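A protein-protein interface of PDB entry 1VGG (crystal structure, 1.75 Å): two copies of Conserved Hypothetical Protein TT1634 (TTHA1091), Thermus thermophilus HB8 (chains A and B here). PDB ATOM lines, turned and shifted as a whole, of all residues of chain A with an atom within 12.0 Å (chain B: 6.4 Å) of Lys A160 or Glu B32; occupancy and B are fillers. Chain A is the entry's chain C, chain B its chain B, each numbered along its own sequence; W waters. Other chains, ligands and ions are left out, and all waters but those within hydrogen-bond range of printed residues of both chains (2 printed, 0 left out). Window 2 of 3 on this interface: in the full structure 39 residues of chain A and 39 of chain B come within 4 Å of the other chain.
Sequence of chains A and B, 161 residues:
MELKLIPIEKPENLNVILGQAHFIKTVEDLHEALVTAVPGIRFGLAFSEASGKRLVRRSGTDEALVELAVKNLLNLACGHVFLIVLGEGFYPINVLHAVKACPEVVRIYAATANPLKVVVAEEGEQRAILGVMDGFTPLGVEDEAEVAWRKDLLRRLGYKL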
ATOM      1  N   ILE A  93      21.669   1.623  -9.290  1.00  0.00           N
ATOM      2  CA  ILE A  93      20.982   2.326 -10.377  1.00  0.00           C
ATOM      3  C   ILE A  93      21.564   3.723 -10.586  1.00  0.00           C
ATOM      4  O   ILE A  93      21.459   4.282 -11.685  1.00  0.00           O
ATOM      5  CB  ILE A  93      19.441   2.463 -10.155  1.00  0.00           C
ATOM      6  CG1 ILE A  93      19.152   3.183  -8.841  1.00  0.00           C
ATOM      7  CG2 ILE A  93      18.764   1.076 -10.229  1.00  0.00           C
ATOM      8  CD1 ILE A  93      17.663   3.475  -8.639  1.00  0.00           C
ATOM      9  N   VAL A 147       0.709  -6.705  -7.440  1.00  0.00           N
ATOM     10  CA  VAL A 147       1.062  -5.826  -8.550  1.00  0.00           C
ATOM     11  C   VAL A 147       0.758  -4.398  -8.077  1.00  0.00           C
ATOM     12  O   VAL A 147       1.565  -3.476  -8.235  1.00  0.00           O
ATOM     13  CB  VAL A 147       0.220  -6.138  -9.821  1.00  0.00           C
ATOM     14  CG1 VAL A 147       0.416  -5.049 -10.857  1.00  0.00           C
ATOM     15  CG2 VAL A 147       0.621  -7.493 -10.404  1.00  0.00           C
ATOM     16  N   ALA A 148      -0.421  -4.227  -7.487  1.00  0.00           N
ATOM     17  CA  ALA A 148      -0.836  -2.929  -6.990  1.00  0.00           C
ATOM     18  C   ALA A 148       0.147  -2.453  -5.923  1.00  0.00           C
ATOM     19  O   ALA A 148       0.482  -1.269  -5.857  1.00  0.00           O
ATOM     20  CB  ALA A 148      -2.256  -3.017  -6.417  1.00  0.00           C
ATOM     21  N   TRP A 149       0.618  -3.377  -5.097  1.00  0.00           N
ATOM     22  CA  TRP A 149       1.568  -3.030  -4.049  1.00  0.00           C
ATOM     23  C   TRP A 149       2.905  -2.518  -4.594  1.00  0.00           C
ATOM     24  O   TRP A 149       3.428  -1.514  -4.103  1.00  0.00           O
ATOM     25  CB  TRP A 149       1.842  -4.233  -3.144  1.00  0.00           C
ATOM     26  CG  TRP A 149       2.912  -3.959  -2.120  1.00  0.00           C
ATOM     27  CD1 TRP A 149       2.751  -3.352  -0.905  1.00  0.00           C
ATOM     28  CD2 TRP A 149       4.313  -4.247  -2.241  1.00  0.00           C
ATOM     29  NE1 TRP A 149       3.964  -3.246  -0.261  1.00  0.00           N
ATOM     30  CE2 TRP A 149       4.939  -3.787  -1.059  1.00  0.00           C
ATOM     31  CE3 TRP A 149       5.100  -4.848  -3.234  1.00  0.00           C
ATOM     32  CZ2 TRP A 149       6.317  -3.911  -0.842  1.00  0.00           C
ATOM     33  CZ3 TRP A 149       6.471  -4.971  -3.019  1.00  0.00           C
ATOM     34  CH2 TRP A 149       7.065  -4.504  -1.832  1.00  0.00           C
ATOM     35  N   ARG A 150       3.472  -3.206  -5.587  1.00  0.00           N
ATOM     36  CA  ARG A 150       4.760  -2.766  -6.124  1.00  0.00           C
ATOM     37  C   ARG A 150       4.643  -1.467  -6.906  1.00  0.00           C
ATOM     38  O   ARG A 150       5.612  -0.715  -7.022  1.00  0.00           O
ATOM     39  CB  ARG A 150       5.420  -3.856  -6.990  1.00  0.00           C
ATOM     40  CG  ARG A 150       4.740  -4.179  -8.315  1.00  0.00           C
ATOM     41  CD  ARG A 150       5.670  -5.059  -9.160  1.00  0.00           C
ATOM     42  NE  ARG A 150       4.991  -5.729 -10.269  1.00  0.00           N
ATOM     43  CZ  ARG A 150       4.637  -5.153 -11.412  1.00  0.00           C
ATOM     44  NH1 ARG A 150       4.887  -3.864 -11.634  1.00  0.00           N
ATOM     45  NH2 ARG A 150       4.040  -5.877 -12.350  1.00  0.00           N
ATOM     46  N   LYS A 151       3.459  -1.195  -7.441  1.00  0.00           N
ATOM     47  CA  LYS A 151       3.256   0.045  -8.172  1.00  0.00           C
ATOM     48  C   LYS A 151       3.188   1.173  -7.146  1.00  0.00           C
ATOM     49  O   LYS A 151       3.805   2.216  -7.319  1.00  0.00           O
ATOM     50  CB  LYS A 151       1.966  -0.023  -8.991  1.00  0.00           C
ATOM     51  CG  LYS A 151       2.026  -1.069 -10.098  1.00  0.00           C
ATOM     52  CD  LYS A 151       0.797  -1.038 -10.989  1.00  0.00           C
ATOM     53  CE  LYS A 151       0.646   0.318 -11.645  1.00  0.00           C
ATOM     54  NZ  LYS A 151       1.905   0.724 -12.324  1.00  0.00           N
ATOM     55  N   ASP A 152       2.459   0.935  -6.061  1.00  0.00           N
ATOM     56  CA  ASP A 152       2.312   1.920  -4.991  1.00  0.00           C
ATOM     57  C   ASP A 152       3.656   2.237  -4.348  1.00  0.00           C
ATOM     58  O   ASP A 152       3.960   3.397  -4.051  1.00  0.00           O
ATOM     59  CB  ASP A 152       1.348   1.389  -3.926  1.00  0.00           C
ATOM     60  CG  ASP A 152       1.178   2.351  -2.765  1.00  0.00           C
ATOM     61  OD1 ASP A 152       0.547   3.413  -2.948  1.00  0.00           O
ATOM     62  OD2 ASP A 152       1.690   2.041  -1.672  1.00  0.00           O
ATOM     63  N   LEU A 153       4.461   1.202  -4.126  1.00  0.00           N
ATOM     64  CA  LEU A 153       5.772   1.380  -3.518  1.00  0.00           C
ATOM     65  C   LEU A 153       6.636   2.382  -4.284  1.00  0.00           C
ATOM     66  O   LEU A 153       7.218   3.288  -3.686  1.00  0.00           O
ATOM     67  CB  LEU A 153       6.509   0.043  -3.441  1.00  0.00           C
ATOM     68  CG  LEU A 153       7.974   0.112  -3.000  1.00  0.00           C
ATOM     69  CD1 LEU A 153       8.062   0.531  -1.534  1.00  0.00           C
ATOM     70  CD2 LEU A 153       8.625  -1.241  -3.205  1.00  0.00           C
ATOM     71  N   LEU A 154       6.722   2.228  -5.604  1.00  0.00           N
ATOM     72  CA  LEU A 154       7.545   3.143  -6.398  1.00  0.00           C
ATOM     73  C   LEU A 154       7.054   4.587  -6.379  1.00  0.00           C
ATOM     74  O   LEU A 154       7.855   5.515  -6.522  1.00  0.00           O
ATOM     75  CB  LEU A 154       7.656   2.657  -7.849  1.00  0.00           C
ATOM     76  CG  LEU A 154       8.340   1.303  -8.070  1.00  0.00           C
ATOM     77  CD1 LEU A 154       8.406   1.044  -9.581  1.00  0.00           C
ATOM     78  CD2 LEU A 154       9.753   1.295  -7.459  1.00  0.00           C
ATOM     79  N   ARG A 155       5.746   4.794  -6.226  1.00  0.00           N
ATOM     80  CA  ARG A 155       5.222   6.157  -6.171  1.00  0.00           C
ATOM     81  C   ARG A 155       5.526   6.754  -4.803  1.00  0.00           C
ATOM     82  O   ARG A 155       5.834   7.943  -4.688  1.00  0.00           O
ATOM     83  CB  ARG A 155       3.709   6.195  -6.429  1.00  0.00           C
ATOM     84  CG  ARG A 155       3.330   6.202  -7.903  1.00  0.00           C
ATOM     85  CD  ARG A 155       3.422   4.809  -8.474  1.00  0.00           C
ATOM     86  NE  ARG A 155       3.315   4.755  -9.933  1.00  0.00           N
ATOM     87  CZ  ARG A 155       3.729   3.709 -10.645  1.00  0.00           C
ATOM     88  NH1 ARG A 155       4.254   2.671 -10.007  1.00  0.00           N
ATOM     89  NH2 ARG A 155       3.646   3.701 -11.975  1.00  0.00           N
ATOM     90  N   ARG A 156       5.439   5.930  -3.763  1.00  0.00           N
ATOM     91  CA  ARG A 156       5.740   6.401  -2.416  1.00  0.00           C
ATOM     92  C   ARG A 156       7.215   6.753  -2.303  1.00  0.00           C
ATOM     93  O   ARG A 156       7.583   7.689  -1.590  1.00  0.00           O
ATOM     94  CB  ARG A 156       5.392   5.334  -1.372  1.00  0.00           C
ATOM     95  CG  ARG A 156       3.910   5.075  -1.226  1.00  0.00           C
ATOM     96  CD  ARG A 156       3.636   4.097  -0.094  1.00  0.00           C
ATOM     97  NE  ARG A 156       2.222   3.747  -0.006  1.00  0.00           N
ATOM     98  CZ  ARG A 156       1.249   4.600   0.300  1.00  0.00           C
ATOM     99  NH1 ARG A 156       1.528   5.871   0.554  1.00  0.00           N
ATOM    100  NH2 ARG A 156      -0.008   4.181   0.348  1.00  0.00           N
ATOM    101  N   LEU A 157       8.054   5.997  -3.008  1.00  0.00           N
ATOM    102  CA  LEU A 157       9.500   6.220  -3.000  1.00  0.00           C
ATOM    103  C   LEU A 157       9.912   7.388  -3.879  1.00  0.00           C
ATOM    104  O   LEU A 157      11.037   7.878  -3.780  1.00  0.00           O
ATOM    105  CB  LEU A 157      10.238   4.966  -3.472  1.00  0.00           C
ATOM    106  CG  LEU A 157      10.255   3.778  -2.511  1.00  0.00           C
ATOM    107  CD1 LEU A 157      10.917   2.594  -3.178  1.00  0.00           C
ATOM    108  CD2 LEU A 157      10.989   4.167  -1.241  1.00  0.00           C
ATOM    109  N   GLY A 158       9.005   7.826  -4.744  1.00  0.00           N
ATOM    110  CA  GLY A 158       9.311   8.940  -5.623  1.00  0.00           C
ATOM    111  C   GLY A 158      10.000   8.561  -6.921  1.00  0.00           C
ATOM    112  O   GLY A 158      10.501   9.442  -7.621  1.00  0.00           O
ATOM    113  N   TYR A 159      10.026   7.268  -7.251  1.00  0.00           N
ATOM    114  CA  TYR A 159      10.656   6.806  -8.495  1.00  0.00           C
ATOM    115  C   TYR A 159       9.691   6.818  -9.676  1.00  0.00           C
ATOM    116  O   TYR A 159      10.109   6.800 -10.830  1.00  0.00           O
ATOM    117  CB  TYR A 159      11.233   5.389  -8.336  1.00  0.00           C
ATOM    118  CG  TYR A 159      12.560   5.342  -7.610  1.00  0.00           C
ATOM    119  CD1 TYR A 159      12.676   4.716  -6.377  1.00  0.00           C
ATOM    120  CD2 TYR A 159      13.693   5.954  -8.149  1.00  0.00           C
ATOM    121  CE1 TYR A 159      13.879   4.696  -5.690  1.00  0.00           C
ATOM    122  CE2 TYR A 159      14.908   5.940  -7.471  1.00  0.00           C
ATOM    123  CZ  TYR A 159      14.991   5.310  -6.239  1.00  0.00           C
ATOM    124  OH  TYR A 159      16.177   5.310  -5.539  1.00  0.00           O
ATOM    125  N   LYS A 160       8.396   6.833  -9.382  1.00  0.00           N
ATOM    126  CA  LYS A 160       7.368   6.873 -10.418  1.00  0.00           C
ATOM    127  C   LYS A 160       6.349   7.923  -9.984  1.00  0.00           C
ATOM    128  O   LYS A 160       6.154   8.143  -8.782  1.00  0.00           O
ATOM    129  CB  LYS A 160       6.681   5.508 -10.563  1.00  0.00           C
ATOM    130  CG  LYS A 160       7.557   4.414 -11.168  1.00  0.00           C
ATOM    131  CD  LYS A 160       7.946   4.726 -12.614  1.00  0.00           C
ATOM    132  CE  LYS A 160       8.953   3.706 -13.134  1.00  0.00           C
ATOM    133  NZ  LYS A 160       9.322   3.940 -14.562  1.00  0.00           N
ATOM    134  N   LEU A 161       5.710   8.574 -10.949  1.00  0.00           N
ATOM    135  CA  LEU A 161       4.729   9.605 -10.638  1.00  0.00           C
ATOM    136  C   LEU A 161       3.288   9.121 -10.797  1.00  0.00           C
ATOM    137  O   LEU A 161       3.083   8.029 -11.358  1.00  0.00           O
ATOM    138  CB  LEU A 161       4.960  10.835 -11.528  1.00  0.00           C
ATOM    139  CG  LEU A 161       6.323  11.538 -11.455  1.00  0.00           C
ATOM    140  CD1 LEU A 161       6.711  11.751  -9.993  1.00  0.00           C
ATOM    141  CD2 LEU A 161       7.384  10.709 -12.164  1.00  0.00           C
ATOM    142  OXT LEU A 161       2.374   9.847 -10.359  1.00  0.00           O
ATOM    143  N   LYS B  25      11.936  -1.988  -9.582  1.00  0.00           N
ATOM    144  CA  LYS B  25      11.627  -1.047 -10.659  1.00  0.00           C
ATOM    145  C   LYS B  25      11.993  -1.614 -12.031  1.00  0.00           C
ATOM    146  O   LYS B  25      11.648  -1.041 -13.063  1.00  0.00           O
ATOM    147  CB  LYS B  25      12.353   0.285 -10.415  1.00  0.00           C
ATOM    148  CG  LYS B  25      11.881   1.427 -11.326  1.00  0.00           C
ATOM    149  CD  LYS B  25      12.206   2.802 -10.716  1.00  0.00           C
ATOM    150  CE  LYS B  25      13.684   3.188 -10.843  1.00  0.00           C
ATOM    151  NZ  LYS B  25      14.010   3.743 -12.195  1.00  0.00           N
ATOM    152  N   VAL B  27      10.735  -4.074 -13.605  1.00  0.00           N
ATOM    153  CA  VAL B  27       9.544  -4.377 -14.398  1.00  0.00           C
ATOM    154  C   VAL B  27       8.963  -3.194 -15.167  1.00  0.00           C
ATOM    155  O   VAL B  27       8.836  -3.236 -16.392  1.00  0.00           O
ATOM    156  CB  VAL B  27       8.449  -4.994 -13.509  1.00  0.00           C
ATOM    157  CG1 VAL B  27       7.246  -5.377 -14.361  1.00  0.00           C
ATOM    158  CG2 VAL B  27       9.010  -6.212 -12.775  1.00  0.00           C
ATOM    159  N   GLU B  28       8.595  -2.133 -14.459  1.00  0.00           N
ATOM    160  CA  GLU B  28       8.051  -0.985 -15.158  1.00  0.00           C
ATOM    161  C   GLU B  28       9.085  -0.342 -16.075  1.00  0.00           C
ATOM    162  O   GLU B  28       8.743   0.088 -17.175  1.00  0.00           O
ATOM    163  CB  GLU B  28       7.522   0.053 -14.167  1.00  0.00           C
ATOM    164  CG  GLU B  28       6.288  -0.407 -13.409  1.00  0.00           C
ATOM    165  CD  GLU B  28       5.660   0.709 -12.594  1.00  0.00           C
ATOM    166  OE1 GLU B  28       5.351   0.466 -11.413  1.00  0.00           O
ATOM    167  OE2 GLU B  28       5.468   1.821 -13.134  1.00  0.00           O
ATOM    168  N   ASP B  29      10.346  -0.272 -15.645  1.00  0.00           N
ATOM    169  CA  ASP B  29      11.361   0.353 -16.498  1.00  0.00           C
ATOM    170  C   ASP B  29      11.576  -0.400 -17.807  1.00  0.00           C
ATOM    171  O   ASP B  29      11.684   0.217 -18.869  1.00  0.00           O
ATOM    172  CB  ASP B  29      12.707   0.487 -15.761  1.00  0.00           C
ATOM    173  CG  ASP B  29      12.770   1.716 -14.865  1.00  0.00           C
ATOM    174  OD1 ASP B  29      11.754   2.428 -14.744  1.00  0.00           O
ATOM    175  OD2 ASP B  29      13.844   1.970 -14.277  1.00  0.00           O
ATOM    176  N   LEU B  30      11.644  -1.726 -17.756  1.00  0.00           N
ATOM    177  CA  LEU B  30      11.865  -2.456 -19.002  1.00  0.00           C
ATOM    178  C   LEU B  30      10.642  -2.397 -19.905  1.00  0.00           C
ATOM    179  O   LEU B  30      10.771  -2.275 -21.123  1.00  0.00           O
ATOM    180  CB  LEU B  30      12.259  -3.913 -18.728  1.00  0.00           C
ATOM    181  CG  LEU B  30      13.725  -4.136 -18.324  1.00  0.00           C
ATOM    182  CD1 LEU B  30      13.951  -5.629 -18.051  1.00  0.00           C
ATOM    183  CD2 LEU B  30      14.668  -3.655 -19.452  1.00  0.00           C
ATOM    184  N   HIS B  31       9.456  -2.480 -19.314  1.00  0.00           N
ATOM    185  CA  HIS B  31       8.219  -2.398 -20.093  1.00  0.00           C
ATOM    186  C   HIS B  31       8.209  -1.060 -20.845  1.00  0.00           C
ATOM    187  O   HIS B  31       7.947  -1.013 -22.048  1.00  0.00           O
ATOM    188  CB  HIS B  31       6.998  -2.488 -19.166  1.00  0.00           C
ATOM    189  CG  HIS B  31       5.682  -2.509 -19.885  1.00  0.00           C
ATOM    190  ND1 HIS B  31       4.766  -3.530 -19.728  1.00  0.00           N
ATOM    191  CD2 HIS B  31       5.126  -1.635 -20.756  1.00  0.00           C
ATOM    192  CE1 HIS B  31       3.703  -3.281 -20.473  1.00  0.00           C
ATOM    193  NE2 HIS B  31       3.897  -2.137 -21.108  1.00  0.00           N
ATOM    194  N   GLU B  32       8.519   0.021 -20.132  1.00  0.00           N
ATOM    195  CA  GLU B  32       8.543   1.351 -20.737  1.00  0.00           C
ATOM    196  C   GLU B  32       9.640   1.479 -21.795  1.00  0.00           C
ATOM    197  O   GLU B  32       9.442   2.104 -22.837  1.00  0.00           O
ATOM    198  CB  GLU B  32       8.760   2.427 -19.665  1.00  0.00           C
ATOM    199  CG  GLU B  32       7.619   2.564 -18.676  1.00  0.00           C
ATOM    200  CD  GLU B  32       7.838   3.706 -17.702  1.00  0.00           C
ATOM    201  OE1 GLU B  32       8.434   4.723 -18.112  1.00  0.00           O
ATOM    202  OE2 GLU B  32       7.398   3.592 -16.540  1.00  0.00           O
ATOM    203  N   ALA B  33      10.800   0.899 -21.524  1.00  0.00           N
ATOM    204  CA  ALA B  33      11.899   0.973 -22.477  1.00  0.00           C
ATOM    205  C   ALA B  33      11.503   0.291 -23.786  1.00  0.00           C
ATOM    206  O   ALA B  33      11.804   0.779 -24.872  1.00  0.00           O
ATOM    207  CB  ALA B  33      13.140   0.316 -21.898  1.00  0.00           C
ATOM    208  N   LEU B  34      10.823  -0.840 -23.673  1.00  0.00           N
ATOM    209  CA  LEU B  34      10.400  -1.583 -24.852  1.00  0.00           C
ATOM    210  C   LEU B  34       9.353  -0.853 -25.694  1.00  0.00           C
ATOM    211  O   LEU B  34       9.491  -0.755 -26.919  1.00  0.00           O
ATOM    212  CB  LEU B  34       9.878  -2.957 -24.432  1.00  0.00           C
ATOM    213  CG  LEU B  34      10.934  -3.906 -23.859  1.00  0.00           C
ATOM    214  CD1 LEU B  34      10.245  -5.147 -23.276  1.00  0.00           C
ATOM    215  CD2 LEU B  34      11.917  -4.314 -24.963  1.00  0.00           C
ATOM    216  N   VAL B  35       8.313  -0.329 -25.051  1.00  0.00           N
ATOM    217  CA  VAL B  35       7.264   0.368 -25.797  1.00  0.00           C
ATOM    218  C   VAL B  35       7.730   1.713 -26.343  1.00  0.00           C
ATOM    219  O   VAL B  35       7.140   2.242 -27.286  1.00  0.00           O
ATOM    220  CB  VAL B  35       5.973   0.576 -24.944  1.00  0.00           C
ATOM    221  CG1 VAL B  35       5.423  -0.766 -24.511  1.00  0.00           C
ATOM    222  CG2 VAL B  35       6.251   1.471 -23.750  1.00  0.00           C
ATOM    223  N   THR B  36       8.784   2.264 -25.750  1.00  0.00           N
ATOM    224  CA  THR B  36       9.328   3.529 -26.228  1.00  0.00           C
ATOM    225  C   THR B  36      10.237   3.286 -27.441  1.00  0.00           C
ATOM    226  O   THR B  36      10.351   4.143 -28.327  1.00  0.00           O
ATOM    227  CB  THR B  36      10.121   4.248 -25.114  1.00  0.00           C
ATOM    228  OG1 THR B  36       9.222   4.608 -24.057  1.00  0.00           O
ATOM    229  CG2 THR B  36      10.788   5.517 -25.646  1.00  0.00           C
ATOM    230  N   ALA B  37      10.859   2.108 -27.489  1.00  0.00           N
ATOM    231  CA  ALA B  37      11.771   1.750 -28.581  1.00  0.00           C
ATOM    232  C   ALA B  37      11.082   1.376 -29.892  1.00  0.00           C
ATOM    233  O   ALA B  37      11.557   1.729 -30.984  1.00  0.00           O
ATOM    234  CB  ALA B  37      12.672   0.604 -28.145  1.00  0.00           C
ATOM    235  N   PHE B  43       5.086  -8.006 -26.463  1.00  0.00           N
ATOM    236  CA  PHE B  43       6.062  -8.776 -25.701  1.00  0.00           C
ATOM    237  C   PHE B  43       5.509  -9.198 -24.347  1.00  0.00           C
ATOM    238  O   PHE B  43       4.443  -8.744 -23.918  1.00  0.00           O
ATOM    239  CB  PHE B  43       7.313  -7.931 -25.433  1.00  0.00           C
ATOM    240  CG  PHE B  43       7.052  -6.735 -24.558  1.00  0.00           C
ATOM    241  CD1 PHE B  43       6.586  -5.543 -25.106  1.00  0.00           C
ATOM    242  CD2 PHE B  43       7.203  -6.825 -23.175  1.00  0.00           C
ATOM    243  CE1 PHE B  43       6.271  -4.452 -24.286  1.00  0.00           C
ATOM    244  CE2 PHE B  43       6.887  -5.743 -22.345  1.00  0.00           C
ATOM    245  CZ  PHE B  43       6.421  -4.558 -22.903  1.00  0.00           C
HETATM  246  O   HOH W   1      11.829   5.717 -12.548  1.00  0.00           O
HETATM  247  O   HOH W   2       6.049  -1.575 -10.032  1.00  0.00           O
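The side-chain hydroxyl (OG1) of Thr B36 lies within hydrogen-bond range of the backbone carbonyl oxygen (O) of Glu B32 (2.8 Å). The backbone carbonyl oxygen of Leu A154 lies within hydrogen-bond range of the backbone NH of Lys A160. The backbone carbonyl oxygen of Lys A151 lies within hydrogen-bond range of the guanidinium group of Arg A155, 2.8 Å away. The side-chain amino group of Lys B25 lies within salt-bridge range of the side-chain carboxylate of Asp B29 (2.7 Å). The backbone carbonyl oxygen of Leu A154 is in hydrogen-bond range of the backbone NH of Tyr A159, 2.9 Å away. NE of Arg A155 is in salt-bridge range of O of Leu A161 (3.6 Å).
Among the printed residues, pairs that only touch across the chains: Arg A150 with Val B27 (3.8 Å), Leu A154 with Lys B25 (3.9 Å), Leu A154 with Glu B28 (3.6 Å), Tyr A159 with Lys B25 (3.6 Å) and Lys A160 with Glu B28 (3.9 Å).
Of the printed residues of chain B, Arg A150 touches Val B27 (3.8 Å). Printed residues of chain B within 4 Å of Lys A151: Glu B28 (3.6 Å). Of the printed residues of chain B, Arg A155 touches Glu B28 (2.8 Å). Of chain B, only Glu B28 (3.9 Å), Asp B29 (2.9 Å) and Glu B32 (2.8 Å) come within 4 Å of Lys A160. Of chain A, only Leu A154 and Tyr A159 come within 4 Å of Lys B25. Of the printed residues of chain A, Val B27 touches Arg A150. Glu B28 touches four residues of chain A. Of chain A, only Lys A160 (2.9 Å) comes within 4 Å of Asp B29. No residue of chain A comes within 4 Å of His B31. Of chain A, only Lys A160 (2.8 Å) comes within 4 Å of Glu B32. No residue of chain A comes within 4 Å of Ala B33. No residue of chain A comes within 4 Å of Val B35. No residue of chain A comes within 4 Å of Thr B36.
No position is printed for both chains. Of the 9 pairs that touch across the chains among the printed residues, none has its exchanged pair printed and touching as well.
Hydrophobic or aromatic side chains of chain A that line the printed part of chain B: Leu A154 and Tyr A159. Of the 13 printed residues of chain B, 5 touch a printed residue of chain A.
Water W2 bridges the side-chain carboxylate of Glu B28 (2.6 Å) and the guanidinium group of Arg A150 (3.0 Å). Water W1 bridges O of Tyr A159 (2.7 Å) and NZ of Lys B25 (3.0 Å).
NZ of Lys A160 lies within salt-bridge range of OE2 of Glu B32 (2.8 Å). OE1 of Glu B28 lies within salt-bridge range of NZ of Lys A151 (3.6 Å). OD1 of Asp B29 lies within salt-bridge range of NZ of Lys A160 (2.9 Å). The side-chain carboxylate (OE1) of Glu B28 lies within salt-bridge range of the guanidinium group (NH1) of Arg A155, 2.8 Å away.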
